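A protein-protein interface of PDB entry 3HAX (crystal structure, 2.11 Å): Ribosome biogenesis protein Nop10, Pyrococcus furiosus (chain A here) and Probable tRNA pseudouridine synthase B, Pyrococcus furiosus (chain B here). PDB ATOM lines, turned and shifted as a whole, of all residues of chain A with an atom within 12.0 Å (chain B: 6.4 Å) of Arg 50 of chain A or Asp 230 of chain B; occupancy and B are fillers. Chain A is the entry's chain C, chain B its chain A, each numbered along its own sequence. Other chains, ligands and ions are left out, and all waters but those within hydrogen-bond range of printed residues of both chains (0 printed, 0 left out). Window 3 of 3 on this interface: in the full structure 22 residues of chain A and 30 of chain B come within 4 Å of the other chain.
The backbone NH (N) of Asp 230 of chain B is in hydrogen-bond range of the backbone carbonyl oxygen (O) of Tyr 225 of chain B, at 3.3 Å. The backbone NH of Gly 231 of chain B lies within hydrogen-bond range of the backbone carbonyl oxygen of Phe 226 of chain B. The backbone carbonyl oxygen (O) of Phe 226 of chain B is in hydrogen-bond range of the backbone NH (N) of Ile 232 of chain B, 2.9 Å away. The side-chain carboxylate of Asp 39 of chain A is in salt-bridge range of the guanidinium group of Arg 45 of chain A. O of Arg 46 of chain A sits close to NH1 of Arg 50 of chain A (3.4 Å). The backbone NH (N) of Ile 55 of chain A sits at hydrogen-bond distance from the backbone carbonyl oxygen (O) of Arg 50 of chain A, 2.8 Å away.
Hydrophobic or aromatic side chains of chain B that line the printed part of chain A: Tyr 225 and Phe 226. Along chain B the printed residues that touch a printed residue of chain A span positions 222 to 230. Hydrophobic or aromatic side chains of chain A that line the printed part of chain B: Leu 53 and Ile 55. Among the printed residues, 9 pairs touch across the chains.
NH2 of Arg 45 of chain A lies within salt-bridge range of OD1 of Asp 222 of chain B (2.8 Å). OD1 of Asp 222 of chain B is in salt-bridge range of NH2 of Arg 46 of chain A (2.9 Å). The side-chain carboxylate (OD2) of Asp 222 of chain B is in salt-bridge range of the side-chain amino group (NZ) of Lys 49 of chain A (2.7 Å). The side-chain carboxylate (OD1) of Asp 230 of chain B is in salt-bridge range of the guanidinium group (NE) of Arg 50 of chain A.
Among the printed residues, merely in contact across the chains: Arg 46 of chain A with Tyr 225 of chain B (3.7 Å), Arg 46 of chain A with Phe 226 of chain B (3.98 Å), Arg 50 of chain A with Phe 226 of chain B (3.7 Å), Leu 53 of chain A with Phe 226 of chain B (3.8 Å) and Ile 55 of chain A with Phe 226 of chain B (3.8 Å).
Tyr 41 of chain A touches none of the printed residues of chain B. Printed residues of chain B within 4 Å of Arg 45 of chain A: Asp 222. Arg 50 of chain A touches just these residues of chain B: Phe 226 (3.7 Å) and Asp 230 (2.6 Å). Glu 51 of chain A touches none of the printed residues of chain B. Of the printed residues of chain B, Leu 53 of chain A touches Phe 226 (3.8 Å). Printed residues of chain B within 4 Å of Ile 55 of chain A: Phe 226 (3.8 Å). Of the printed residues of chain A, Tyr 225 of chain B touches Arg 46. No residue of chain A comes within 4 Å of Glu 229 of chain B. No residue of chain A comes within 4 Å of Gly 231 of chain B. Ile 232 of chain B touches none of the printed residues of chain A. The nearest residue of chain A that does not touch Asp 230 of chain B is Ile 55 of chain A (4.1 Å).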
ATOM      1  N   ASP A  39      16.181  10.038  13.909  1.00  0.00           N
ATOM      2  CA  ASP A  39      14.728   9.900  13.735  1.00  0.00           C
ATOM      3  C   ASP A  39      13.916  10.254  14.992  1.00  0.00           C
ATOM      4  O   ASP A  39      13.252   9.389  15.564  1.00  0.00           O
ATOM      5  CB  ASP A  39      14.400   8.478  13.252  1.00  0.00           C
ATOM      6  CG  ASP A  39      13.062   8.389  12.533  1.00  0.00           C
ATOM      7  OD1 ASP A  39      12.564   9.419  12.024  1.00  0.00           O
ATOM      8  OD2 ASP A  39      12.512   7.269  12.470  1.00  0.00           O
ATOM      9  N   TYR A  41      11.151  11.706  15.666  1.00  0.00           N
ATOM     10  CA  TYR A  41       9.687  11.591  15.673  1.00  0.00           C
ATOM     11  C   TYR A  41       9.175  10.295  15.046  1.00  0.00           C
ATOM     12  O   TYR A  41       8.014  10.205  14.637  1.00  0.00           O
ATOM     13  CB  TYR A  41       9.047  12.834  15.037  1.00  0.00           C
ATOM     14  CG  TYR A  41       9.511  14.100  15.716  1.00  0.00           C
ATOM     15  CD1 TYR A  41      10.476  14.916  15.127  1.00  0.00           C
ATOM     16  CD2 TYR A  41       9.025  14.453  16.973  1.00  0.00           C
ATOM     17  CE1 TYR A  41      10.926  16.062  15.761  1.00  0.00           C
ATOM     18  CE2 TYR A  41       9.470  15.596  17.615  1.00  0.00           C
ATOM     19  CZ  TYR A  41      10.420  16.394  17.004  1.00  0.00           C
ATOM     20  OH  TYR A  41      10.858  17.530  17.634  1.00  0.00           O
ATOM     21  N   GLY A  42      10.047   9.289  15.009  1.00  0.00           N
ATOM     22  CA  GLY A  42       9.714   7.972  14.472  1.00  0.00           C
ATOM     23  C   GLY A  42       8.545   7.304  15.175  1.00  0.00           C
ATOM     24  O   GLY A  42       7.726   6.655  14.527  1.00  0.00           O
ATOM     25  N   GLU A  43       8.471   7.462  16.500  1.00  0.00           N
ATOM     26  CA  GLU A  43       7.377   6.905  17.304  1.00  0.00           C
ATOM     27  C   GLU A  43       6.017   7.421  16.827  1.00  0.00           C
ATOM     28  O   GLU A  43       5.046   6.665  16.743  1.00  0.00           O
ATOM     29  CB  GLU A  43       7.568   7.237  18.793  1.00  0.00           C
ATOM     30  CG  GLU A  43       6.426   6.756  19.693  1.00  0.00           C
ATOM     31  CD  GLU A  43       6.459   7.337  21.102  1.00  0.00           C
ATOM     32  OE1 GLU A  43       5.601   6.937  21.920  1.00  0.00           O
ATOM     33  OE2 GLU A  43       7.332   8.179  21.408  1.00  0.00           O
ATOM     34  N   TYR A  44       5.970   8.708  16.505  1.00  0.00           N
ATOM     35  CA  TYR A  44       4.731   9.376  16.116  1.00  0.00           C
ATOM     36  C   TYR A  44       4.369   9.127  14.656  1.00  0.00           C
ATOM     37  O   TYR A  44       3.189   9.014  14.318  1.00  0.00           O
ATOM     38  CB  TYR A  44       4.819  10.869  16.439  1.00  0.00           C
ATOM     39  CG  TYR A  44       5.144  11.117  17.897  1.00  0.00           C
ATOM     40  CD1 TYR A  44       6.455  11.374  18.308  1.00  0.00           C
ATOM     41  CD2 TYR A  44       4.147  11.058  18.872  1.00  0.00           C
ATOM     42  CE1 TYR A  44       6.759  11.585  19.651  1.00  0.00           C
ATOM     43  CE2 TYR A  44       4.440  11.270  20.215  1.00  0.00           C
ATOM     44  CZ  TYR A  44       5.747  11.531  20.597  1.00  0.00           C
ATOM     45  OH  TYR A  44       6.036  11.741  21.927  1.00  0.00           O
ATOM     46  N   ARG A  45       5.386   9.027  13.800  1.00  0.00           N
ATOM     47  CA  ARG A  45       5.187   8.641  12.405  1.00  0.00           C
ATOM     48  C   ARG A  45       4.686   7.198  12.297  1.00  0.00           C
ATOM     49  O   ARG A  45       3.822   6.903  11.473  1.00  0.00           O
ATOM     50  CB  ARG A  45       6.476   8.821  11.595  1.00  0.00           C
ATOM     51  CG  ARG A  45       6.310   8.543  10.099  1.00  0.00           C
ATOM     52  CD  ARG A  45       7.629   8.595   9.342  1.00  0.00           C
ATOM     53  NE  ARG A  45       8.563   7.550   9.763  1.00  0.00           N
ATOM     54  CZ  ARG A  45       9.672   7.775  10.461  1.00  0.00           C
ATOM     55  NH1 ARG A  45       9.999   9.013  10.816  1.00  0.00           N
ATOM     56  NH2 ARG A  45      10.460   6.765  10.801  1.00  0.00           N
ATOM     57  N   ARG A  46       5.227   6.309  13.130  1.00  0.00           N
ATOM     58  CA  ARG A  46       4.806   4.904  13.139  1.00  0.00           C
ATOM     59  C   ARG A  46       3.382   4.721  13.671  1.00  0.00           C
ATOM     60  O   ARG A  46       2.671   3.809  13.247  1.00  0.00           O
ATOM     61  CB  ARG A  46       5.802   4.029  13.912  1.00  0.00           C
ATOM     62  CG  ARG A  46       7.045   3.684  13.109  1.00  0.00           C
ATOM     63  CD  ARG A  46       7.944   2.659  13.790  1.00  0.00           C
ATOM     64  NE  ARG A  46       8.735   3.229  14.882  1.00  0.00           N
ATOM     65  CZ  ARG A  46       9.855   3.934  14.727  1.00  0.00           C
ATOM     66  NH1 ARG A  46      10.491   4.400  15.794  1.00  0.00           N
ATOM     67  NH2 ARG A  46      10.340   4.184  13.517  1.00  0.00           N
ATOM     68  N   ARG A  47       2.970   5.595  14.587  1.00  0.00           N
ATOM     69  CA  ARG A  47       1.609   5.578  15.126  1.00  0.00           C
ATOM     70  C   ARG A  47       0.603   5.933  14.032  1.00  0.00           C
ATOM     71  O   ARG A  47      -0.479   5.344  13.949  1.00  0.00           O
ATOM     72  CB  ARG A  47       1.490   6.546  16.308  1.00  0.00           C
ATOM     73  CG  ARG A  47       0.242   6.359  17.159  1.00  0.00           C
ATOM     74  CD  ARG A  47       0.404   7.022  18.518  1.00  0.00           C
ATOM     75  NE  ARG A  47       1.428   6.362  19.329  1.00  0.00           N
ATOM     76  CZ  ARG A  47       2.080   6.931  20.339  1.00  0.00           C
ATOM     77  NH1 ARG A  47       1.828   8.190  20.682  1.00  0.00           N
ATOM     78  NH2 ARG A  47       2.991   6.238  21.012  1.00  0.00           N
ATOM     79  N   TRP A  48       0.977   6.898  13.198  1.00  0.00           N
ATOM     80  CA  TRP A  48       0.198   7.271  12.026  1.00  0.00           C
ATOM     81  C   TRP A  48       0.177   6.124  11.016  1.00  0.00           C
ATOM     82  O   TRP A  48      -0.883   5.757  10.508  1.00  0.00           O
ATOM     83  CB  TRP A  48       0.777   8.549  11.409  1.00  0.00           C
ATOM     84  CG  TRP A  48       0.468   8.761   9.953  1.00  0.00           C
ATOM     85  CD1 TRP A  48      -0.743   9.071   9.406  1.00  0.00           C
ATOM     86  CD2 TRP A  48       1.398   8.700   8.864  1.00  0.00           C
ATOM     87  NE1 TRP A  48      -0.628   9.200   8.042  1.00  0.00           N
ATOM     88  CE2 TRP A  48       0.675   8.977   7.682  1.00  0.00           C
ATOM     89  CE3 TRP A  48       2.772   8.434   8.770  1.00  0.00           C
ATOM     90  CZ2 TRP A  48       1.278   8.996   6.417  1.00  0.00           C
ATOM     91  CZ3 TRP A  48       3.375   8.454   7.511  1.00  0.00           C
ATOM     92  CH2 TRP A  48       2.625   8.733   6.353  1.00  0.00           C
ATOM     93  N   LYS A  49       1.351   5.549  10.762  1.00  0.00           N
ATOM     94  CA  LYS A  49       1.525   4.503   9.755  1.00  0.00           C
ATOM     95  C   LYS A  49       0.763   3.220  10.095  1.00  0.00           C
ATOM     96  O   LYS A  49       0.163   2.608   9.213  1.00  0.00           O
ATOM     97  CB  LYS A  49       3.014   4.218   9.546  1.00  0.00           C
ATOM     98  CG  LYS A  49       3.347   3.509   8.244  1.00  0.00           C
ATOM     99  CD  LYS A  49       4.844   3.564   7.943  1.00  0.00           C
ATOM    100  CE  LYS A  49       5.259   4.911   7.354  1.00  0.00           C
ATOM    101  NZ  LYS A  49       6.701   4.934   6.961  1.00  0.00           N
ATOM    102  N   ARG A  50       0.781   2.828  11.368  1.00  0.00           N
ATOM    103  CA  ARG A  50       0.036   1.650  11.828  1.00  0.00           C
ATOM    104  C   ARG A  50      -1.470   1.793  11.606  1.00  0.00           C
ATOM    105  O   ARG A  50      -2.139   0.825  11.234  1.00  0.00           O
ATOM    106  CB  ARG A  50       0.324   1.346  13.303  1.00  0.00           C
ATOM    107  CG  ARG A  50       1.656   0.657  13.550  1.00  0.00           C
ATOM    108  CD  ARG A  50       1.802   0.221  15.004  1.00  0.00           C
ATOM    109  NE  ARG A  50       3.203   0.012  15.356  1.00  0.00           N
ATOM    110  CZ  ARG A  50       3.996   0.945  15.876  1.00  0.00           C
ATOM    111  NH1 ARG A  50       3.530   2.161  16.127  1.00  0.00           N
ATOM    112  NH2 ARG A  50       5.259   0.659  16.150  1.00  0.00           N
ATOM    113  N   GLU A  51      -1.995   2.996  11.833  1.00  0.00           N
ATOM    114  CA  GLU A  51      -3.415   3.275  11.608  1.00  0.00           C
ATOM    115  C   GLU A  51      -3.756   3.233  10.115  1.00  0.00           C
ATOM    116  O   GLU A  51      -4.814   2.733   9.732  1.00  0.00           O
ATOM    117  CB  GLU A  51      -3.814   4.622  12.227  1.00  0.00           C
ATOM    118  CG  GLU A  51      -5.327   4.848  12.322  1.00  0.00           C
ATOM    119  CD  GLU A  51      -5.709   6.102  13.102  1.00  0.00           C
ATOM    120  OE1 GLU A  51      -4.865   7.012  13.248  1.00  0.00           O
ATOM    121  OE2 GLU A  51      -6.868   6.182  13.565  1.00  0.00           O
ATOM    122  N   VAL A  52      -2.851   3.753   9.286  1.00  0.00           N
ATOM    123  CA  VAL A  52      -3.011   3.742   7.828  1.00  0.00           C
ATOM    124  C   VAL A  52      -2.974   2.313   7.278  1.00  0.00           C
ATOM    125  O   VAL A  52      -3.827   1.927   6.474  1.00  0.00           O
ATOM    126  CB  VAL A  52      -1.929   4.617   7.124  1.00  0.00           C
ATOM    127  CG1 VAL A  52      -1.938   4.408   5.610  1.00  0.00           C
ATOM    128  CG2 VAL A  52      -2.129   6.088   7.453  1.00  0.00           C
ATOM    129  N   LEU A  53      -1.991   1.536   7.730  1.00  0.00           N
ATOM    130  CA  LEU A  53      -1.795   0.166   7.256  1.00  0.00           C
ATOM    131  C   LEU A  53      -2.787  -0.833   7.855  1.00  0.00           C
ATOM    132  O   LEU A  53      -3.060  -1.873   7.254  1.00  0.00           O
ATOM    133  CB  LEU A  53      -0.354  -0.293   7.513  1.00  0.00           C
ATOM    134  CG  LEU A  53       0.764   0.363   6.692  1.00  0.00           C
ATOM    135  CD1 LEU A  53       2.128  -0.049   7.219  1.00  0.00           C
ATOM    136  CD2 LEU A  53       0.646   0.029   5.205  1.00  0.00           C
ATOM    137  N   GLY A  54      -3.314  -0.515   9.036  1.00  0.00           N
ATOM    138  CA  GLY A  54      -4.287  -1.371   9.714  1.00  0.00           C
ATOM    139  C   GLY A  54      -3.680  -2.306  10.747  1.00  0.00           C
ATOM    140  O   GLY A  54      -4.279  -3.328  11.094  1.00  0.00           O
ATOM    141  N   ILE A  55      -2.492  -1.955  11.234  1.00  0.00           N
ATOM    142  CA  ILE A  55      -1.805  -2.737  12.263  1.00  0.00           C
ATOM    143  C   ILE A  55      -2.357  -2.398  13.648  1.00  0.00           C
ATOM    144  O   ILE A  55      -2.477  -1.226  14.011  1.00  0.00           O
ATOM    145  CB  ILE A  55      -0.273  -2.507  12.237  1.00  0.00           C
ATOM    146  CG1 ILE A  55       0.288  -2.767  10.832  1.00  0.00           C
ATOM    147  CG2 ILE A  55       0.424  -3.387  13.283  1.00  0.00           C
ATOM    148  CD1 ILE A  55       1.685  -2.205  10.598  1.00  0.00           C
ATOM    149  N   ASP B 222      10.777   1.829   9.463  1.00  0.00           N
ATOM    150  CA  ASP B 222       9.471   1.584  10.069  1.00  0.00           C
ATOM    151  C   ASP B 222       9.085   0.111   9.967  1.00  0.00           C
ATOM    152  O   ASP B 222       8.606  -0.474  10.941  1.00  0.00           O
ATOM    153  CB  ASP B 222       8.398   2.491   9.460  1.00  0.00           C
ATOM    154  CG  ASP B 222       8.520   3.937   9.928  1.00  0.00           C
ATOM    155  OD1 ASP B 222       9.354   4.221  10.812  1.00  0.00           O
ATOM    156  OD2 ASP B 222       7.775   4.796   9.417  1.00  0.00           O
ATOM    157  N   TYR B 225      11.119  -1.926  12.483  1.00  0.00           N
ATOM    158  CA  TYR B 225      10.539  -1.877  13.827  1.00  0.00           C
ATOM    159  C   TYR B 225       9.170  -2.551  13.940  1.00  0.00           C
ATOM    160  O   TYR B 225       8.788  -2.987  15.025  1.00  0.00           O
ATOM    161  CB  TYR B 225      10.497  -0.440  14.366  1.00  0.00           C
ATOM    162  CG  TYR B 225      11.868   0.108  14.707  1.00  0.00           C
ATOM    163  CD1 TYR B 225      12.402   1.190  14.010  1.00  0.00           C
ATOM    164  CD2 TYR B 225      12.642  -0.475  15.714  1.00  0.00           C
ATOM    165  CE1 TYR B 225      13.671   1.689  14.311  1.00  0.00           C
ATOM    166  CE2 TYR B 225      13.912   0.014  16.022  1.00  0.00           C
ATOM    167  CZ  TYR B 225      14.417   1.095  15.315  1.00  0.00           C
ATOM    168  OH  TYR B 225      15.670   1.582  15.620  1.00  0.00           O
ATOM    169  N   PHE B 226       8.439  -2.645  12.829  1.00  0.00           N
ATOM    170  CA  PHE B 226       7.212  -3.444  12.794  1.00  0.00           C
ATOM    171  C   PHE B 226       7.538  -4.928  13.007  1.00  0.00           C
ATOM    172  O   PHE B 226       6.762  -5.658  13.624  1.00  0.00           O
ATOM    173  CB  PHE B 226       6.430  -3.242  11.485  1.00  0.00           C
ATOM    174  CG  PHE B 226       5.831  -1.858  11.320  1.00  0.00           C
ATOM    175  CD1 PHE B 226       5.409  -1.424  10.068  1.00  0.00           C
ATOM    176  CD2 PHE B 226       5.700  -0.990  12.404  1.00  0.00           C
ATOM    177  CE1 PHE B 226       4.855  -0.153   9.894  1.00  0.00           C
ATOM    178  CE2 PHE B 226       5.152   0.283  12.242  1.00  0.00           C
ATOM    179  CZ  PHE B 226       4.729   0.702  10.982  1.00  0.00           C
ATOM    180  N   TRP B 227       8.691  -5.361  12.499  1.00  0.00           N
ATOM    181  CA  TRP B 227       9.196  -6.706  12.764  1.00  0.00           C
ATOM    182  C   TRP B 227       9.788  -6.817  14.172  1.00  0.00           C
ATOM    183  O   TRP B 227       9.316  -7.609  14.991  1.00  0.00           O
ATOM    184  CB  TRP B 227      10.225  -7.111  11.700  1.00  0.00           C
ATOM    185  CG  TRP B 227      10.984  -8.371  12.018  1.00  0.00           C
ATOM    186  CD1 TRP B 227      10.466  -9.561  12.449  1.00  0.00           C
ATOM    187  CD2 TRP B 227      12.401  -8.568  11.910  1.00  0.00           C
ATOM    188  NE1 TRP B 227      11.472 -10.479  12.628  1.00  0.00           N
ATOM    189  CE2 TRP B 227      12.669  -9.898  12.303  1.00  0.00           C
ATOM    190  CE3 TRP B 227      13.468  -7.748  11.523  1.00  0.00           C
ATOM    191  CZ2 TRP B 227      13.960 -10.429  12.319  1.00  0.00           C
ATOM    192  CZ3 TRP B 227      14.753  -8.275  11.541  1.00  0.00           C
ATOM    193  CH2 TRP B 227      14.987  -9.605  11.938  1.00  0.00           C
ATOM    194  N   LYS B 228      10.818  -6.015  14.437  1.00  0.00           N
ATOM    195  CA  LYS B 228      11.528  -6.003  15.716  1.00  0.00           C
ATOM    196  C   LYS B 228      10.624  -5.828  16.936  1.00  0.00           C
ATOM    197  O   LYS B 228      10.706  -6.602  17.892  1.00  0.00           O
ATOM    198  CB  LYS B 228      12.588  -4.894  15.704  1.00  0.00           C
ATOM    199  CG  LYS B 228      14.043  -5.350  15.622  1.00  0.00           C
ATOM    200  CD  LYS B 228      14.238  -6.642  14.852  1.00  0.00           C
ATOM    201  CE  LYS B 228      15.644  -7.175  15.048  1.00  0.00           C
ATOM    202  NZ  LYS B 228      15.962  -7.449  16.481  1.00  0.00           N
ATOM    203  N   GLU B 229       9.760  -4.819  16.896  1.00  0.00           N
ATOM    204  CA  GLU B 229       9.011  -4.411  18.081  1.00  0.00           C
ATOM    205  C   GLU B 229       7.535  -4.812  18.076  1.00  0.00           C
ATOM    206  O   GLU B 229       6.954  -5.038  19.140  1.00  0.00           O
ATOM    207  CB  GLU B 229       9.192  -2.909  18.333  1.00  0.00           C
ATOM    208  CG  GLU B 229      10.654  -2.523  18.583  1.00  0.00           C
ATOM    209  CD  GLU B 229      10.868  -1.045  18.876  1.00  0.00           C
ATOM    210  OE1 GLU B 229      11.931  -0.710  19.445  1.00  0.00           O
ATOM    211  OE2 GLU B 229       9.990  -0.221  18.540  1.00  0.00           O
ATOM    212  N   ASP B 230       6.943  -4.925  16.888  1.00  0.00           N
ATOM    213  CA  ASP B 230       5.555  -5.377  16.750  1.00  0.00           C
ATOM    214  C   ASP B 230       5.441  -6.883  16.494  1.00  0.00           C
ATOM    215  O   ASP B 230       4.387  -7.473  16.722  1.00  0.00           O
ATOM    216  CB  ASP B 230       4.840  -4.610  15.632  1.00  0.00           C
ATOM    217  CG  ASP B 230       4.755  -3.117  15.895  1.00  0.00           C
ATOM    218  OD1 ASP B 230       3.976  -2.446  15.191  1.00  0.00           O
ATOM    219  OD2 ASP B 230       5.458  -2.608  16.792  1.00  0.00           O
ATOM    220  N   GLY B 231       6.521  -7.494  16.011  1.00  0.00           N
ATOM    221  CA  GLY B 231       6.547  -8.931  15.736  1.00  0.00           C
ATOM    222  C   GLY B 231       5.914  -9.316  14.410  1.00  0.00           C
ATOM    223  O   GLY B 231       5.520 -10.466  14.215  1.00  0.00           O
ATOM    224  N   ILE B 232       5.820  -8.349  13.501  1.00  0.00           N
ATOM    225  CA  ILE B 232       5.221  -8.556  12.185  1.00  0.00           C
ATOM    226  C   ILE B 232       6.324  -8.617  11.130  1.00  0.00           C
ATOM    227  O   ILE B 232       6.975  -7.611  10.845  1.00  0.00           O
ATOM    228  CB  ILE B 232       4.216  -7.419  11.830  1.00  0.00           C
ATOM    229  CG1 ILE B 232       3.193  -7.193  12.960  1.00  0.00           C
ATOM    230  CG2 ILE B 232       3.540  -7.680  10.482  1.00  0.00           C
ATOM    231  CD1 ILE B 232       2.321  -8.397  13.312  1.00  0.00           C
